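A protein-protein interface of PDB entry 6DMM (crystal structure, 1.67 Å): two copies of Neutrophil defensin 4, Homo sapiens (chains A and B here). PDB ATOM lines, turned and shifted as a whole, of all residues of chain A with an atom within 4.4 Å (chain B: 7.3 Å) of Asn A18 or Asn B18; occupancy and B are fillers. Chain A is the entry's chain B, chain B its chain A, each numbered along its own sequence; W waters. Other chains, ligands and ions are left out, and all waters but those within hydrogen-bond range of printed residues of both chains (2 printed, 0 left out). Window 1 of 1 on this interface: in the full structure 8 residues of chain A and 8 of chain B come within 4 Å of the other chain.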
ATOM      1  N   ARG A  15      24.364  17.182  37.261  1.00  0.00           N
ATOM      2  CA  ARG A  15      24.561  17.915  36.019  1.00  0.00           C
ATOM      3  C   ARG A  15      24.367  16.987  34.823  1.00  0.00           C
ATOM      4  O   ARG A  15      24.984  15.917  34.762  1.00  0.00           O
ATOM      5  CB  ARG A  15      25.957  18.524  36.004  1.00  0.00           C
ATOM      6  CG  ARG A  15      26.206  19.386  34.797  1.00  0.00           C
ATOM      7  CD  ARG A  15      27.599  19.965  34.797  1.00  0.00           C
ATOM      8  NE  ARG A  15      27.858  20.620  33.526  1.00  0.00           N
ATOM      9  CZ  ARG A  15      28.145  19.991  32.388  1.00  0.00           C
ATOM     10  NH1 ARG A  15      28.241  18.667  32.340  1.00  0.00           N
ATOM     11  NH2 ARG A  15      28.341  20.697  31.285  1.00  0.00           N
ATOM     12  N   GLY A  17      24.154  18.602  31.522  1.00  0.00           N
ATOM     13  CA  GLY A  17      24.691  19.330  30.388  1.00  0.00           C
ATOM     14  C   GLY A  17      24.631  20.821  30.662  1.00  0.00           C
ATOM     15  O   GLY A  17      24.599  21.241  31.816  1.00  0.00           O
ATOM     16  N   ASN A  18      24.597  21.607  29.587  1.00  0.00           N
ATOM     17  CA  ASN A  18      24.534  23.065  29.662  1.00  0.00           C
ATOM     18  C   ASN A  18      23.164  23.517  29.181  1.00  0.00           C
ATOM     19  O   ASN A  18      22.544  22.850  28.346  1.00  0.00           O
ATOM     20  CB  ASN A  18      25.617  23.742  28.788  1.00  0.00           C
ATOM     21  CG  ASN A  18      27.041  23.188  29.008  1.00  0.00           C
ATOM     22  OD1 ASN A  18      27.593  23.287  30.117  1.00  0.00           O
ATOM     23  ND2 ASN A  18      27.612  22.575  27.981  1.00  0.00           N
ATOM     24  N   CYS A  19      22.659  24.649  29.729  1.00  0.00           N
ATOM     25  CA  CYS A  19      21.587  25.408  29.078  1.00  0.00           C
ATOM     26  C   CYS A  19      22.191  26.718  28.577  1.00  0.00           C
ATOM     27  O   CYS A  19      22.622  27.565  29.363  1.00  0.00           O
ATOM     28  CB  CYS A  19      20.378  25.625  29.990  1.00  0.00           C
ATOM     29  SG  CYS A  19      20.848  25.842  31.690  1.00  0.00           S
ATOM     30  N   LEU A  20      22.275  26.853  27.261  1.00  0.00           N
ATOM     31  CA  LEU A  20      22.903  28.004  26.623  1.00  0.00           C
ATOM     32  C   LEU A  20      21.837  29.049  26.330  1.00  0.00           C
ATOM     33  O   LEU A  20      20.951  28.824  25.487  1.00  0.00           O
ATOM     34  CB  LEU A  20      23.601  27.574  25.330  1.00  0.00           C
ATOM     35  CG  LEU A  20      24.320  28.699  24.597  1.00  0.00           C
ATOM     36  CD1 LEU A  20      25.597  29.058  25.311  1.00  0.00           C
ATOM     37  CD2 LEU A  20      24.641  28.239  23.159  1.00  0.00           C
ATOM     38  N   PHE A  26      24.654  28.298  31.113  1.00  0.00           N
ATOM     39  CA  PHE A  26      24.196  27.882  32.423  1.00  0.00           C
ATOM     40  C   PHE A  26      24.280  26.349  32.546  1.00  0.00           C
ATOM     41  O   PHE A  26      24.606  25.624  31.599  1.00  0.00           O
ATOM     42  CB  PHE A  26      22.761  28.368  32.685  1.00  0.00           C
ATOM     43  CG  PHE A  26      22.587  29.873  32.656  1.00  0.00           C
ATOM     44  CD1 PHE A  26      22.636  30.594  31.458  1.00  0.00           C
ATOM     45  CD2 PHE A  26      22.326  30.560  33.829  1.00  0.00           C
ATOM     46  CE1 PHE A  26      22.495  31.987  31.465  1.00  0.00           C
ATOM     47  CE2 PHE A  26      22.148  31.927  33.836  1.00  0.00           C
ATOM     48  CZ  PHE A  26      22.242  32.644  32.660  1.00  0.00           C
ATOM     49  N   TYR A  28      22.619  22.709  33.320  1.00  0.00           N
ATOM     50  CA  TYR A  28      21.358  21.963  33.296  1.00  0.00           C
ATOM     51  C   TYR A  28      21.398  20.808  34.298  1.00  0.00           C
ATOM     52  O   TYR A  28      22.225  19.902  34.165  1.00  0.00           O
ATOM     53  CB  TYR A  28      21.022  21.417  31.897  1.00  0.00           C
ATOM     54  CG  TYR A  28      19.507  21.329  31.747  1.00  0.00           C
ATOM     55  CD1 TYR A  28      18.719  22.453  31.930  1.00  0.00           C
ATOM     56  CD2 TYR A  28      18.873  20.139  31.441  1.00  0.00           C
ATOM     57  CE1 TYR A  28      17.332  22.395  31.795  1.00  0.00           C
ATOM     58  CE2 TYR A  28      17.463  20.074  31.319  1.00  0.00           C
ATOM     59  CZ  TYR A  28      16.719  21.195  31.512  1.00  0.00           C
ATOM     60  OH  TYR A  28      15.341  21.161  31.416  1.00  0.00           O
ATOM     61  N   CYS B   4      13.324  20.821  27.320  1.00  0.00           N
ATOM     62  CA  CYS B   4      14.230  20.601  26.194  1.00  0.00           C
ATOM     63  C   CYS B   4      13.530  19.743  25.155  1.00  0.00           C
ATOM     64  O   CYS B   4      13.174  18.587  25.430  1.00  0.00           O
ATOM     65  CB  CYS B   4      15.536  19.933  26.624  1.00  0.00           C
ATOM     66  SG  CYS B   4      16.414  20.815  27.919  1.00  0.00           S
ATOM     67  N   ARG B  15      10.982  30.206  22.418  1.00  0.00           N
ATOM     68  CA  ARG B  15      12.324  29.659  22.268  1.00  0.00           C
ATOM     69  C   ARG B  15      13.303  30.559  23.009  1.00  0.00           C
ATOM     70  O   ARG B  15      13.433  31.746  22.670  1.00  0.00           O
ATOM     71  CB  ARG B  15      12.651  29.586  20.781  1.00  0.00           C
ATOM     72  CG  ARG B  15      13.938  28.919  20.459  1.00  0.00           C
ATOM     73  CD  ARG B  15      14.017  28.601  18.980  1.00  0.00           C
ATOM     74  NE  ARG B  15      14.430  29.733  18.149  1.00  0.00           N
ATOM     75  CZ  ARG B  15      13.940  29.999  16.935  1.00  0.00           C
ATOM     76  NH1 ARG B  15      12.999  29.226  16.399  1.00  0.00           N
ATOM     77  NH2 ARG B  15      14.396  31.044  16.249  1.00  0.00           N
ATOM     78  N   VAL B  16      13.981  30.021  24.024  1.00  0.00           N
ATOM     79  CA  VAL B  16      14.873  30.825  24.849  1.00  0.00           C
ATOM     80  C   VAL B  16      16.324  30.401  24.738  1.00  0.00           C
ATOM     81  O   VAL B  16      17.201  31.137  25.222  1.00  0.00           O
ATOM     82  CB  VAL B  16      14.439  30.820  26.328  1.00  0.00           C
ATOM     83  CG1 VAL B  16      12.951  31.128  26.440  1.00  0.00           C
ATOM     84  CG2 VAL B  16      14.775  29.497  26.932  1.00  0.00           C
ATOM     85  N   GLY B  17      16.610  29.256  24.127  1.00  0.00           N
ATOM     86  CA  GLY B  17      17.997  28.867  23.902  1.00  0.00           C
ATOM     87  C   GLY B  17      18.137  27.399  23.575  1.00  0.00           C
ATOM     88  O   GLY B  17      17.305  26.836  22.854  1.00  0.00           O
ATOM     89  N   ASN B  18      19.179  26.763  24.104  1.00  0.00           N
ATOM     90  CA  ASN B  18      19.476  25.378  23.792  1.00  0.00           C
ATOM     91  C   ASN B  18      19.846  24.611  25.054  1.00  0.00           C
ATOM     92  O   ASN B  18      20.426  25.167  25.989  1.00  0.00           O
ATOM     93  CB  ASN B  18      20.629  25.297  22.771  1.00  0.00           C
ATOM     94  CG  ASN B  18      20.284  25.978  21.480  1.00  0.00           C
ATOM     95  OD1 ASN B  18      19.614  25.403  20.621  1.00  0.00           O
ATOM     96  ND2 ASN B  18      20.727  27.208  21.330  1.00  0.00           N
ATOM     97  N   CYS B  19      19.481  23.322  25.078  1.00  0.00           N
ATOM     98  CA  CYS B  19      20.011  22.353  26.024  1.00  0.00           C
ATOM     99  C   CYS B  19      21.086  21.538  25.321  1.00  0.00           C
ATOM    100  O   CYS B  19      20.799  20.846  24.340  1.00  0.00           O
ATOM    101  CB  CYS B  19      18.909  21.422  26.506  1.00  0.00           C
ATOM    102  SG  CYS B  19      17.416  22.291  26.931  1.00  0.00           S
ATOM    103  N   LEU B  20      22.301  21.624  25.821  1.00  0.00           N
ATOM    104  CA  LEU B  20      23.420  20.852  25.296  1.00  0.00           C
ATOM    105  C   LEU B  20      23.594  19.626  26.178  1.00  0.00           C
ATOM    106  O   LEU B  20      24.114  19.724  27.293  1.00  0.00           O
ATOM    107  CB  LEU B  20      24.699  21.682  25.276  1.00  0.00           C
ATOM    108  CG  LEU B  20      24.548  23.068  24.652  1.00  0.00           C
ATOM    109  CD1 LEU B  20      25.908  23.801  24.750  1.00  0.00           C
ATOM    110  CD2 LEU B  20      24.017  22.979  23.179  1.00  0.00           C
ATOM    111  N   ILE B  21      23.176  18.473  25.672  1.00  0.00           N
ATOM    112  CA  ILE B  21      23.208  17.244  26.436  1.00  0.00           C
ATOM    113  C   ILE B  21      23.899  16.204  25.582  1.00  0.00           C
ATOM    114  O   ILE B  21      23.391  15.873  24.502  1.00  0.00           O
ATOM    115  CB  ILE B  21      21.801  16.792  26.853  1.00  0.00           C
ATOM    116  CG1 ILE B  21      21.228  17.832  27.822  1.00  0.00           C
ATOM    117  CG2 ILE B  21      21.847  15.482  27.615  1.00  0.00           C
ATOM    118  CD1 ILE B  21      19.710  17.714  28.006  1.00  0.00           C
ATOM    119  N   GLY B  22      25.059  15.729  26.056  1.00  0.00           N
ATOM    120  CA  GLY B  22      25.875  14.747  25.332  1.00  0.00           C
ATOM    121  C   GLY B  22      26.230  15.323  23.973  1.00  0.00           C
ATOM    122  O   GLY B  22      26.735  16.445  23.872  1.00  0.00           O
ATOM    123  N   VAL B  24      24.099  16.171  21.633  1.00  0.00           N
ATOM    124  CA  VAL B  24      22.893  16.692  21.002  1.00  0.00           C
ATOM    125  C   VAL B  24      22.673  18.132  21.450  1.00  0.00           C
ATOM    126  O   VAL B  24      22.848  18.453  22.623  1.00  0.00           O
ATOM    127  CB  VAL B  24      21.672  15.821  21.336  1.00  0.00           C
ATOM    128  CG1 VAL B  24      20.597  16.096  20.321  1.00  0.00           C
ATOM    129  CG2 VAL B  24      22.041  14.349  21.341  1.00  0.00           C
ATOM    130  N   SER B  25      22.358  19.007  20.514  1.00  0.00           N
ATOM    131  CA  SER B  25      21.855  20.332  20.865  1.00  0.00           C
ATOM    132  C   SER B  25      20.330  20.313  20.743  1.00  0.00           C
ATOM    133  O   SER B  25      19.795  20.214  19.633  1.00  0.00           O
ATOM    134  CB  SER B  25      22.473  21.382  19.959  1.00  0.00           C
ATOM    135  OG  SER B  25      21.897  22.631  20.243  1.00  0.00           O
ATOM    136  N   PHE B  26      19.627  20.374  21.879  1.00  0.00           N
ATOM    137  CA  PHE B  26      18.174  20.417  21.901  1.00  0.00           C
ATOM    138  C   PHE B  26      17.752  21.879  22.005  1.00  0.00           C
ATOM    139  O   PHE B  26      18.570  22.747  22.307  1.00  0.00           O
ATOM    140  CB  PHE B  26      17.625  19.599  23.090  1.00  0.00           C
ATOM    141  CG  PHE B  26      17.989  18.107  23.051  1.00  0.00           C
ATOM    142  CD1 PHE B  26      17.330  17.228  22.187  1.00  0.00           C
ATOM    143  CD2 PHE B  26      18.952  17.591  23.919  1.00  0.00           C
ATOM    144  CE1 PHE B  26      17.639  15.841  22.169  1.00  0.00           C
ATOM    145  CE2 PHE B  26      19.281  16.240  23.902  1.00  0.00           C
ATOM    146  CZ  PHE B  26      18.631  15.363  23.015  1.00  0.00           C
ATOM    147  N   THR B  27      16.460  22.137  21.809  1.00  0.00           N
ATOM    148  CA  THR B  27      15.926  23.489  21.843  1.00  0.00           C
ATOM    149  C   THR B  27      15.328  23.663  23.228  1.00  0.00           C
ATOM    150  O   THR B  27      14.661  22.745  23.721  1.00  0.00           O
ATOM    151  CB  THR B  27      14.883  23.705  20.740  1.00  0.00           C
ATOM    152  OG1 THR B  27      15.469  23.343  19.478  1.00  0.00           O
ATOM    153  CG2 THR B  27      14.487  25.157  20.653  1.00  0.00           C
ATOM    154  N   TYR B  28      15.674  24.776  23.901  1.00  0.00           N
ATOM    155  CA  TYR B  28      15.149  25.113  25.232  1.00  0.00           C
ATOM    156  C   TYR B  28      13.960  26.050  25.054  1.00  0.00           C
ATOM    157  O   TYR B  28      14.100  27.146  24.497  1.00  0.00           O
ATOM    158  CB  TYR B  28      16.239  25.745  26.122  1.00  0.00           C
ATOM    159  CG  TYR B  28      15.954  25.790  27.626  1.00  0.00           C
ATOM    160  CD1 TYR B  28      15.268  24.759  28.272  1.00  0.00           C
ATOM    161  CD2 TYR B  28      16.409  26.856  28.405  1.00  0.00           C
ATOM    162  CE1 TYR B  28      14.974  24.825  29.675  1.00  0.00           C
ATOM    163  CE2 TYR B  28      16.134  26.925  29.804  1.00  0.00           C
ATOM    164  CZ  TYR B  28      15.427  25.917  30.420  1.00  0.00           C
ATOM    165  OH  TYR B  28      15.160  25.997  31.776  1.00  0.00           O
ATOM    166  N   CYS B  29      12.794  25.598  25.528  1.00  0.00           N
ATOM    167  CA  CYS B  29      11.475  26.172  25.291  1.00  0.00           C
ATOM    168  C   CYS B  29      10.786  26.438  26.617  1.00  0.00           C
ATOM    169  O   CYS B  29      10.816  25.589  27.509  1.00  0.00           O
ATOM    170  CB  CYS B  29      10.580  25.200  24.499  1.00  0.00           C
ATOM    171  SG  CYS B  29      11.414  24.612  23.027  1.00  0.00           S
HETATM  172  O   HOH W   1      27.102  19.443  27.305  1.00  0.00           O
HETATM  173  O   HOH W   2      13.937  19.366  30.145  1.00  0.00           O
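The backbone carbonyl oxygen of Tyr B28 lies within hydrogen-bond range of the backbone NH of Val B16 (2.9 Å). The backbone NH (N) of Tyr B28 is in hydrogen-bond range of the backbone carbonyl oxygen (O) of Gly B17 (2.8 Å). The side-chain amide oxygen (OD1) of Asn B18 sits close to the backbone carbonyl oxygen (O) of Phe B26, at 3.3 Å. The backbone carbonyl oxygen (O) of Cys B19 sits at hydrogen-bond distance from the backbone NH (N) of Phe B26, 2.8 Å away. OD1 of Asn A18 lies within hydrogen-bond range of NH2 of Arg A15. The backbone NH of Phe A26 is in hydrogen-bond range of the backbone carbonyl oxygen of Cys A19.
Gly A17 touches Leu B20, and with the chains exchanged Leu A20 touches Gly B17. Asn A18 touches its own counterpart, Asn B18. Asn A18 touches Cys B19, and with the chains exchanged Cys A19 touches Asn B18. Asn A18 touches Leu B20, and with the chains exchanged Leu A20 touches Asn B18. 7 positions are printed for both chains. Of the 9 pairs that touch across the chains among the printed residues, 8 have their exchanged pair printed and touching as well.
Asn A18 touches just these residues of chain B: Asn B18 (3.9 Å), Cys B19 (3.5 Å) and Leu B20 (2.8 Å). Of the printed residues of chain B, Cys A19 touches Asn B18 (3.3 Å). Printed residues of chain A within 4 Å of Cys B4: Tyr A28 (3.6 Å). Asn B18 touches just these residues of chain A: Asn A18 (3.9 Å), Cys A19 (3.3 Å) and Leu A20 (2.8 Å). Printed residues of chain A within 4 Å of Cys B19: Asn A18. Printed residues of chain A within 4 Å of Leu B20: Gly A17 (3.2 Å) and Asn A18 (2.8 Å). Val B24 touches none of the printed residues of chain A. Of the printed residues of chain A, Tyr B28 touches Tyr A28 (3.99 Å). The nearest printed residue of chain A that does not touch Asn B18 is Tyr A28 (6.8 Å).
Water W2 bridges OH of Tyr A28 and N of Cys B4. Water W1 bridges O of Leu B20 (3.0 Å) and ND2 of Asn A18 (3.2 Å).
The side-chain hydroxyl (OH) of Tyr A28 lies close to the side-chain sulfur (SG) of Cys B4, at 3.7 Å. N of Leu A20 sits at hydrogen-bond distance from O of Asn B18, 2.8 Å away. The backbone NH (N) of Leu B20 sits at hydrogen-bond distance from the backbone carbonyl oxygen (O) of Asn A18, at 2.8 Å.
Gly A17 touches Leu B20 (CA to O, 3.2 Å). Asn A18 touches Asn B18. O of Asn A18 touches CA of Cys B19, at 3.5 Å. Cys A19 touches Asn B18 (CA to O, 3.3 Å). Gly B17 touches Leu A20. CE1 of Tyr A28 touches CE1 of Tyr B28, 3.99 Å away.
Printed residues of chain A that touch a printed residue of chain B: Gly A17, Asn A18, Cys A19, Leu A20 and Tyr A28. Among the printed residues, 9 pairs touch across the chains.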
